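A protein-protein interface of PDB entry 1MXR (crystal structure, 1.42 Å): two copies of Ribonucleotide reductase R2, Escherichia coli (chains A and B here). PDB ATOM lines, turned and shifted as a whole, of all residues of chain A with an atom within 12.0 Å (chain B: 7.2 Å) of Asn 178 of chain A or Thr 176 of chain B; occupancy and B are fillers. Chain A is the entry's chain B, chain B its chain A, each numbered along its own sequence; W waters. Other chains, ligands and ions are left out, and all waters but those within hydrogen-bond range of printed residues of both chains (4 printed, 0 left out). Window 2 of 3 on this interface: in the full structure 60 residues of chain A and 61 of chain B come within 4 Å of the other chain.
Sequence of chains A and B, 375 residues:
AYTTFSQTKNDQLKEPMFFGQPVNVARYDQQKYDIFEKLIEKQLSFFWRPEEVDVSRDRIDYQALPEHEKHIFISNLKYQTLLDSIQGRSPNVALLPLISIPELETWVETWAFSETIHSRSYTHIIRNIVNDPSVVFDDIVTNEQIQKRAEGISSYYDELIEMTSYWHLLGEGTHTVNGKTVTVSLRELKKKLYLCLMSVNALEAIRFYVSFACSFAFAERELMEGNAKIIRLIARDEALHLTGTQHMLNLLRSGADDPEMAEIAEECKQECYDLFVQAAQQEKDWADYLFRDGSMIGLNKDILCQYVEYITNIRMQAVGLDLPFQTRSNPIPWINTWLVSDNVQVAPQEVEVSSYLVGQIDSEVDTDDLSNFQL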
ATOM      1  N   TYR A 166     -14.174  31.871 -27.462  1.00  0.00           N
ATOM      2  CA  TYR A 166     -14.850  31.629 -26.181  1.00  0.00           C
ATOM      3  C   TYR A 166     -15.786  32.785 -25.834  1.00  0.00           C
ATOM      4  O   TYR A 166     -16.908  32.557 -25.387  1.00  0.00           O
ATOM      5  CB  TYR A 166     -13.828  31.434 -25.060  1.00  0.00           C
ATOM      6  CG  TYR A 166     -13.325  30.009 -24.948  1.00  0.00           C
ATOM      7  CD1 TYR A 166     -14.170  28.981 -24.536  1.00  0.00           C
ATOM      8  CD2 TYR A 166     -11.990  29.700 -25.250  1.00  0.00           C
ATOM      9  CE1 TYR A 166     -13.672  27.656 -24.427  1.00  0.00           C
ATOM     10  CE2 TYR A 166     -11.510  28.392 -25.138  1.00  0.00           C
ATOM     11  CZ  TYR A 166     -12.367  27.398 -24.729  1.00  0.00           C
ATOM     12  OH  TYR A 166     -11.871  26.109 -24.615  1.00  0.00           O
ATOM     13  N   LEU A 169     -18.854  32.615 -28.093  1.00  0.00           N
ATOM     14  CA  LEU A 169     -19.727  31.470 -27.819  1.00  0.00           C
ATOM     15  C   LEU A 169     -20.379  31.472 -26.442  1.00  0.00           C
ATOM     16  O   LEU A 169     -21.567  31.166 -26.317  1.00  0.00           O
ATOM     17  CB  LEU A 169     -18.954  30.157 -27.989  1.00  0.00           C
ATOM     18  CG  LEU A 169     -18.577  29.771 -29.423  1.00  0.00           C
ATOM     19  CD1 LEU A 169     -17.820  28.459 -29.408  1.00  0.00           C
ATOM     20  CD2 LEU A 169     -19.825  29.654 -30.285  1.00  0.00           C
ATOM     21  N   LEU A 170     -19.614  31.852 -25.425  1.00  0.00           N
ATOM     22  CA  LEU A 170     -20.108  31.783 -24.059  1.00  0.00           C
ATOM     23  C   LEU A 170     -20.316  33.100 -23.339  1.00  0.00           C
ATOM     24  O   LEU A 170     -21.035  33.148 -22.345  1.00  0.00           O
ATOM     25  CB  LEU A 170     -19.142  30.948 -23.216  1.00  0.00           C
ATOM     26  CG  LEU A 170     -18.665  29.576 -23.722  1.00  0.00           C
ATOM     27  CD1 LEU A 170     -17.711  28.942 -22.670  1.00  0.00           C
ATOM     28  CD2 LEU A 170     -19.901  28.700 -23.989  1.00  0.00           C
ATOM     29  N   THR A 174     -17.852  32.667 -15.543  1.00  0.00           N
ATOM     30  CA  THR A 174     -17.108  31.501 -15.102  1.00  0.00           C
ATOM     31  C   THR A 174     -17.941  30.331 -15.599  1.00  0.00           C
ATOM     32  O   THR A 174     -19.033  30.074 -15.102  1.00  0.00           O
ATOM     33  CB  THR A 174     -17.006  31.457 -13.586  1.00  0.00           C
ATOM     34  OG1 THR A 174     -16.329  32.638 -13.134  1.00  0.00           O
ATOM     35  CG2 THR A 174     -16.227  30.225 -13.141  1.00  0.00           C
ATOM     36  N   HIS A 175     -17.401  29.643 -16.592  1.00  0.00           N
ATOM     37  CA  HIS A 175     -18.077  28.537 -17.254  1.00  0.00           C
ATOM     38  C   HIS A 175     -17.425  27.195 -16.958  1.00  0.00           C
ATOM     39  O   HIS A 175     -16.358  27.131 -16.397  1.00  0.00           O
ATOM     40  CB  HIS A 175     -17.996  28.788 -18.775  1.00  0.00           C
ATOM     41  CG  HIS A 175     -18.566  30.103 -19.185  1.00  0.00           C
ATOM     42  ND1 HIS A 175     -17.794  31.152 -19.650  1.00  0.00           N
ATOM     43  CD2 HIS A 175     -19.836  30.560 -19.134  1.00  0.00           C
ATOM     44  CE1 HIS A 175     -18.576  32.196 -19.863  1.00  0.00           C
ATOM     45  NE2 HIS A 175     -19.815  31.868 -19.560  1.00  0.00           N
ATOM     46  N   THR A 176     -18.104  26.121 -17.358  1.00  0.00           N
ATOM     47  CA  THR A 176     -17.484  24.802 -17.258  1.00  0.00           C
ATOM     48  C   THR A 176     -17.528  24.093 -18.604  1.00  0.00           C
ATOM     49  O   THR A 176     -18.528  24.188 -19.345  1.00  0.00           O
ATOM     50  CB  THR A 176     -18.151  23.864 -16.189  1.00  0.00           C
ATOM     51  OG1 THR A 176     -19.551  23.728 -16.444  1.00  0.00           O
ATOM     52  CG2 THR A 176     -17.927  24.427 -14.776  1.00  0.00           C
ATOM     53  N   VAL A 177     -16.452  23.411 -18.919  1.00  0.00           N
ATOM     54  CA  VAL A 177     -16.369  22.641 -20.154  1.00  0.00           C
ATOM     55  C   VAL A 177     -15.721  21.304 -19.814  1.00  0.00           C
ATOM     56  O   VAL A 177     -14.555  21.248 -19.416  1.00  0.00           O
ATOM     57  CB  VAL A 177     -15.494  23.365 -21.225  1.00  0.00           C
ATOM     58  CG1 VAL A 177     -15.335  22.477 -22.454  1.00  0.00           C
ATOM     59  CG2 VAL A 177     -16.125  24.704 -21.605  1.00  0.00           C
ATOM     60  N   ASN A 178     -16.491  20.220 -19.958  1.00  0.00           N
ATOM     61  CA  ASN A 178     -15.952  18.893 -19.652  1.00  0.00           C
ATOM     62  C   ASN A 178     -15.193  18.773 -18.332  1.00  0.00           C
ATOM     63  O   ASN A 178     -14.075  18.232 -18.291  1.00  0.00           O
ATOM     64  CB  ASN A 178     -15.061  18.419 -20.787  1.00  0.00           C
ATOM     65  CG  ASN A 178     -15.826  18.295 -22.111  1.00  0.00           C
ATOM     66  OD1 ASN A 178     -17.008  17.934 -22.129  1.00  0.00           O
ATOM     67  ND2 ASN A 178     -15.142  18.576 -23.230  1.00  0.00           N
ATOM     68  N   GLY A 179     -15.818  19.295 -17.277  1.00  0.00           N
ATOM     69  CA  GLY A 179     -15.251  19.196 -15.955  1.00  0.00           C
ATOM     70  C   GLY A 179     -14.238  20.237 -15.579  1.00  0.00           C
ATOM     71  O   GLY A 179     -13.788  20.270 -14.450  1.00  0.00           O
ATOM     72  N   LYS A 180     -13.906  21.118 -16.513  1.00  0.00           N
ATOM     73  CA  LYS A 180     -12.937  22.181 -16.211  1.00  0.00           C
ATOM     74  C   LYS A 180     -13.585  23.559 -16.173  1.00  0.00           C
ATOM     75  O   LYS A 180     -14.549  23.837 -16.898  1.00  0.00           O
ATOM     76  CB  LYS A 180     -11.837  22.184 -17.270  1.00  0.00           C
ATOM     77  CG  LYS A 180     -10.897  21.008 -17.209  1.00  0.00           C
ATOM     78  CD  LYS A 180      -9.709  21.209 -18.144  1.00  0.00           C
ATOM     79  CE  LYS A 180      -8.746  20.017 -18.080  1.00  0.00           C
ATOM     80  NZ  LYS A 180      -7.476  20.332 -18.794  1.00  0.00           N
ATOM     81  N   THR A 181     -13.065  24.443 -15.325  1.00  0.00           N
ATOM     82  CA  THR A 181     -13.570  25.803 -15.272  1.00  0.00           C
ATOM     83  C   THR A 181     -12.880  26.599 -16.377  1.00  0.00           C
ATOM     84  O   THR A 181     -11.675  26.465 -16.604  1.00  0.00           O
ATOM     85  CB  THR A 181     -13.253  26.460 -13.925  1.00  0.00           C
ATOM     86  OG1 THR A 181     -13.961  25.751 -12.899  1.00  0.00           O
ATOM     87  CG2 THR A 181     -13.687  27.935 -13.916  1.00  0.00           C
ATOM     88  N   VAL A 182     -13.662  27.390 -17.093  1.00  0.00           N
ATOM     89  CA  VAL A 182     -13.131  28.239 -18.158  1.00  0.00           C
ATOM     90  C   VAL A 182     -13.666  29.626 -17.844  1.00  0.00           C
ATOM     91  O   VAL A 182     -14.873  29.844 -17.816  1.00  0.00           O
ATOM     92  CB  VAL A 182     -13.642  27.808 -19.540  1.00  0.00           C
ATOM     93  CG1 VAL A 182     -13.193  28.803 -20.587  1.00  0.00           C
ATOM     94  CG2 VAL A 182     -13.124  26.409 -19.871  1.00  0.00           C
ATOM     95  N   THR A 183     -12.751  30.545 -17.554  1.00  0.00           N
ATOM     96  CA  THR A 183     -13.150  31.906 -17.243  1.00  0.00           C
ATOM     97  C   THR A 183     -12.968  32.804 -18.459  1.00  0.00           C
ATOM     98  O   THR A 183     -11.929  32.779 -19.097  1.00  0.00           O
ATOM     99  CB  THR A 183     -12.322  32.447 -16.053  1.00  0.00           C
ATOM    100  OG1 THR A 183     -12.651  31.690 -14.878  1.00  0.00           O
ATOM    101  CG2 THR A 183     -12.608  33.913 -15.797  1.00  0.00           C
ATOM    102  N   LEU B 170     -13.176  22.732 -29.129  1.00  0.00           N
ATOM    103  CA  LEU B 170     -13.411  21.473 -28.439  1.00  0.00           C
ATOM    104  C   LEU B 170     -13.080  20.211 -29.164  1.00  0.00           C
ATOM    105  O   LEU B 170     -12.878  19.164 -28.512  1.00  0.00           O
ATOM    106  CB  LEU B 170     -14.874  21.426 -28.048  1.00  0.00           C
ATOM    107  CG  LEU B 170     -15.447  22.663 -27.325  1.00  0.00           C
ATOM    108  CD1 LEU B 170     -16.885  22.360 -26.918  1.00  0.00           C
ATOM    109  CD2 LEU B 170     -14.558  23.052 -26.132  1.00  0.00           C
ATOM    110  N   THR B 174     -18.764  14.540 -27.924  1.00  0.00           N
ATOM    111  CA  THR B 174     -19.965  14.992 -27.250  1.00  0.00           C
ATOM    112  C   THR B 174     -19.434  15.580 -25.961  1.00  0.00           C
ATOM    113  O   THR B 174     -18.786  14.895 -25.152  1.00  0.00           O
ATOM    114  CB  THR B 174     -20.921  13.811 -27.016  1.00  0.00           C
ATOM    115  OG1 THR B 174     -21.205  13.225 -28.304  1.00  0.00           O
ATOM    116  CG2 THR B 174     -22.209  14.255 -26.357  1.00  0.00           C
ATOM    117  N   HIS B 175     -19.715  16.865 -25.799  1.00  0.00           N
ATOM    118  CA  HIS B 175     -19.186  17.662 -24.711  1.00  0.00           C
ATOM    119  C   HIS B 175     -20.214  18.160 -23.733  1.00  0.00           C
ATOM    120  O   HIS B 175     -21.407  18.136 -24.024  1.00  0.00           O
ATOM    121  CB  HIS B 175     -18.468  18.867 -25.341  1.00  0.00           C
ATOM    122  CG  HIS B 175     -17.350  18.479 -26.257  1.00  0.00           C
ATOM    123  ND1 HIS B 175     -17.444  18.482 -27.636  1.00  0.00           N
ATOM    124  CD2 HIS B 175     -16.113  18.031 -25.973  1.00  0.00           C
ATOM    125  CE1 HIS B 175     -16.305  18.053 -28.152  1.00  0.00           C
ATOM    126  NE2 HIS B 175     -15.481  17.771 -27.164  1.00  0.00           N
ATOM    127  N   THR B 176     -19.747  18.645 -22.577  1.00  0.00           N
ATOM    128  CA  THR B 176     -20.633  19.194 -21.556  1.00  0.00           C
ATOM    129  C   THR B 176     -20.195  20.649 -21.341  1.00  0.00           C
ATOM    130  O   THR B 176     -19.130  20.908 -20.783  1.00  0.00           O
ATOM    131  CB  THR B 176     -20.532  18.367 -20.260  1.00  0.00           C
ATOM    132  OG1 THR B 176     -20.850  16.998 -20.567  1.00  0.00           O
ATOM    133  CG2 THR B 176     -21.542  18.893 -19.232  1.00  0.00           C
ATOM    134  N   VAL B 177     -21.010  21.576 -21.841  1.00  0.00           N
ATOM    135  CA  VAL B 177     -20.706  23.007 -21.790  1.00  0.00           C
ATOM    136  C   VAL B 177     -21.762  23.713 -20.945  1.00  0.00           C
ATOM    137  O   VAL B 177     -22.934  23.762 -21.317  1.00  0.00           O
ATOM    138  CB  VAL B 177     -20.700  23.571 -23.231  1.00  0.00           C
ATOM    139  CG1 VAL B 177     -20.339  25.090 -23.198  1.00  0.00           C
ATOM    140  CG2 VAL B 177     -19.721  22.788 -24.086  1.00  0.00           C
ATOM    141  N   ASN B 178     -21.345  24.218 -19.784  1.00  0.00           N
ATOM    142  CA  ASN B 178     -22.265  24.849 -18.836  1.00  0.00           C
ATOM    143  C   ASN B 178     -23.467  23.944 -18.545  1.00  0.00           C
ATOM    144  O   ASN B 178     -24.618  24.387 -18.438  1.00  0.00           O
ATOM    145  CB  ASN B 178     -22.714  26.216 -19.357  1.00  0.00           C
ATOM    146  CG  ASN B 178     -21.587  27.236 -19.296  1.00  0.00           C
ATOM    147  OD1 ASN B 178     -20.671  27.091 -18.492  1.00  0.00           O
ATOM    148  ND2 ASN B 178     -21.665  28.277 -20.133  1.00  0.00           N
ATOM    149  N   GLY B 179     -23.177  22.655 -18.424  1.00  0.00           N
ATOM    150  CA  GLY B 179     -24.224  21.703 -18.108  1.00  0.00           C
ATOM    151  C   GLY B 179     -25.117  21.264 -19.259  1.00  0.00           C
ATOM    152  O   GLY B 179     -26.066  20.482 -19.035  1.00  0.00           O
ATOM    153  N   LYS B 180     -24.817  21.762 -20.462  1.00  0.00           N
ATOM    154  CA  LYS B 180     -25.565  21.423 -21.686  1.00  0.00           C
ATOM    155  C   LYS B 180     -24.730  20.431 -22.478  1.00  0.00           C
ATOM    156  O   LYS B 180     -23.503  20.525 -22.510  1.00  0.00           O
ATOM    157  CB  LYS B 180     -25.793  22.675 -22.554  1.00  0.00           C
ATOM    158  CG  LYS B 180     -26.528  23.817 -21.840  1.00  0.00           C
ATOM    159  CD  LYS B 180     -27.794  23.311 -21.161  1.00  0.00           C
ATOM    160  CE  LYS B 180     -28.721  22.607 -22.148  1.00  0.00           C
ATOM    161  NZ  LYS B 180     -29.893  21.962 -21.476  1.00  0.00           N
ATOM    162  N   THR B 181     -25.373  19.467 -23.120  1.00  0.00           N
ATOM    163  CA  THR B 181     -24.637  18.465 -23.884  1.00  0.00           C
ATOM    164  C   THR B 181     -24.552  18.998 -25.291  1.00  0.00           C
ATOM    165  O   THR B 181     -25.571  19.239 -25.917  1.00  0.00           O
ATOM    166  CB  THR B 181     -25.368  17.108 -23.839  1.00  0.00           C
ATOM    167  OG1 THR B 181     -25.462  16.699 -22.459  1.00  0.00           O
ATOM    168  CG2 THR B 181     -24.646  16.074 -24.658  1.00  0.00           C
ATOM    169  N   VAL B 182     -23.323  19.169 -25.770  1.00  0.00           N
ATOM    170  CA  VAL B 182     -23.062  19.747 -27.093  1.00  0.00           C
ATOM    171  C   VAL B 182     -22.301  18.764 -27.974  1.00  0.00           C
ATOM    172  O   VAL B 182     -21.200  18.335 -27.647  1.00  0.00           O
ATOM    173  CB  VAL B 182     -22.213  21.024 -26.950  1.00  0.00           C
ATOM    174  CG1 VAL B 182     -21.841  21.583 -28.333  1.00  0.00           C
ATOM    175  CG2 VAL B 182     -22.982  22.052 -26.135  1.00  0.00           C
HETATM  176  O   HOH W   1     -21.231  25.403 -15.486  1.00  0.00           O
HETATM  177  O   HOH W   2     -20.224  21.809 -18.213  1.00  0.00           O
HETATM  178  O   HOH W   3     -22.696  30.906 -21.780  1.00  0.00           O
HETATM  179  O   HOH W   4     -18.387  15.762 -20.978  1.00  0.00           O
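O of Thr 176 of chain B is in hydrogen-bond range of N of Asn 178 of chain A.
The backbone NH of Asn 178 of chain B is in hydrogen-bond range of the backbone carbonyl oxygen of Thr 176 of chain A (2.9 Å).
Of the 13 printed residues of chain A, 5 touch a printed residue of chain B.
Hydrophobic or aromatic side chains of chain A that line the printed part of chain B: Leu 170, His 175 and Val 177.
Along chain A the printed residues that touch a printed residue of chain B span positions 170 to 178.
Leu 170 of chain A touches Val 177 of chain B, and with the chains exchanged Val 177 of chain A touches Leu 170 of chain B.
His 175 of chain A touches Asn 178 of chain B, and with the chains exchanged Asn 178 of chain A touches His 175 of chain B.
Thr 176 of chain A touches its own counterpart, Thr 176 of chain B.
Thr 176 of chain A touches Val 177 of chain B, and with the chains exchanged Val 177 of chain A touches Thr 176 of chain B.
Of the printed residues of chain B, Asn 178 of chain A touches His 175 and Thr 176.
Of chain A, only Thr 176 (3.6 Å), Val 177 (3.3 Å) and Asn 178 (2.8 Å) come within 4 Å of Thr 176 of chain B.
Of chain A, only Val 177 comes within 4 Å of Leu 170 of chain B.
Of chain A, only Asn 178 comes within 4 Å of His 175 of chain B.
Of chain A, only Leu 170 and Thr 176 come within 4 Å of Val 177 of chain B.
Of chain A, only His 175 (3.1 Å) and Thr 176 (2.9 Å) come within 4 Å of Asn 178 of chain B.
No residue of chain A comes within 4 Å of Gly 179 of chain B.
Val 182 of chain B touches none of the printed residues of chain A.
Of the printed residues of chain B, Val 177 of chain A touches Leu 170 and Thr 176.
Printed residues of chain B within 4 Å of Leu 170 of chain A: Val 177 (3.7 Å).
Printed residues of chain B within 4 Å of His 175 of chain A: Asn 178.
Thr 183 of chain A touches none of the printed residues of chain B.
Tyr 166 of chain A touches none of the printed residues of chain B.
The nearest residue of chain B that does not touch Asn 178 of chain A is Thr 174 of chain B (4.6 Å).
The nearest residue of chain A that does not touch Thr 176 of chain B is Gly 179 of chain A (5.1 Å).
Leu 170 of chain A touches Val 177 of chain B.
His 175 of chain A touches Asn 178 of chain B (CD2 to ND2, 3.1 Å).
Thr 176 of chain A touches Thr 176 of chain B (O to O, 3.6 Å).
CA of Val 177 of chain B touches O of Thr 176 of chain A (3.5 Å).
Leu 170 of chain B touches Val 177 of chain A (CD2 to CG1, 3.8 Å).
Val 177 of chain A touches Thr 176 of chain B (CA to O, 3.3 Å).
His 175 of chain B touches Asn 178 of chain A (CD2 to ND2, 3.0 Å).
Water W1 lies within hydrogen-bond range of the side-chain hydroxyl (OG1) of Thr 176 of chain A (2.6 Å) and the side-chain amide oxygen (OD1) of Asn 178 of chain B (3.5 Å).
Water W2 lies within hydrogen-bond range of OG1 of Thr 176 of chain A (2.7 Å), O of Thr 176 of chain B (2.9 Å), N of Gly 179 of chain B (3.1 Å) and N of Asn 178 of chain B (3.1 Å).
Water W4 bridges OG1 of Thr 176 of chain B and OD1 of Asn 178 of chain A.
Water W3 bridges the backbone carbonyl oxygen of Leu 170 of chain A (2.8 Å) and the side-chain amide nitrogen of Asn 178 of chain B (3.3 Å).
The backbone carbonyl oxygen of Leu 170 of chain B is in hydrogen-bond range of a ring nitrogen (NE2) of His 175 of chain B.
The backbone carbonyl oxygen (O) of His 175 of chain B sits at hydrogen-bond distance from the backbone NH (N) of Val 182 of chain B.
O of Leu 170 of chain A lies within hydrogen-bond range of NE2 of His 175 of chain A.
The backbone NH of Val 182 of chain A sits at hydrogen-bond distance from the backbone carbonyl oxygen of His 175 of chain A (2.8 Å).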
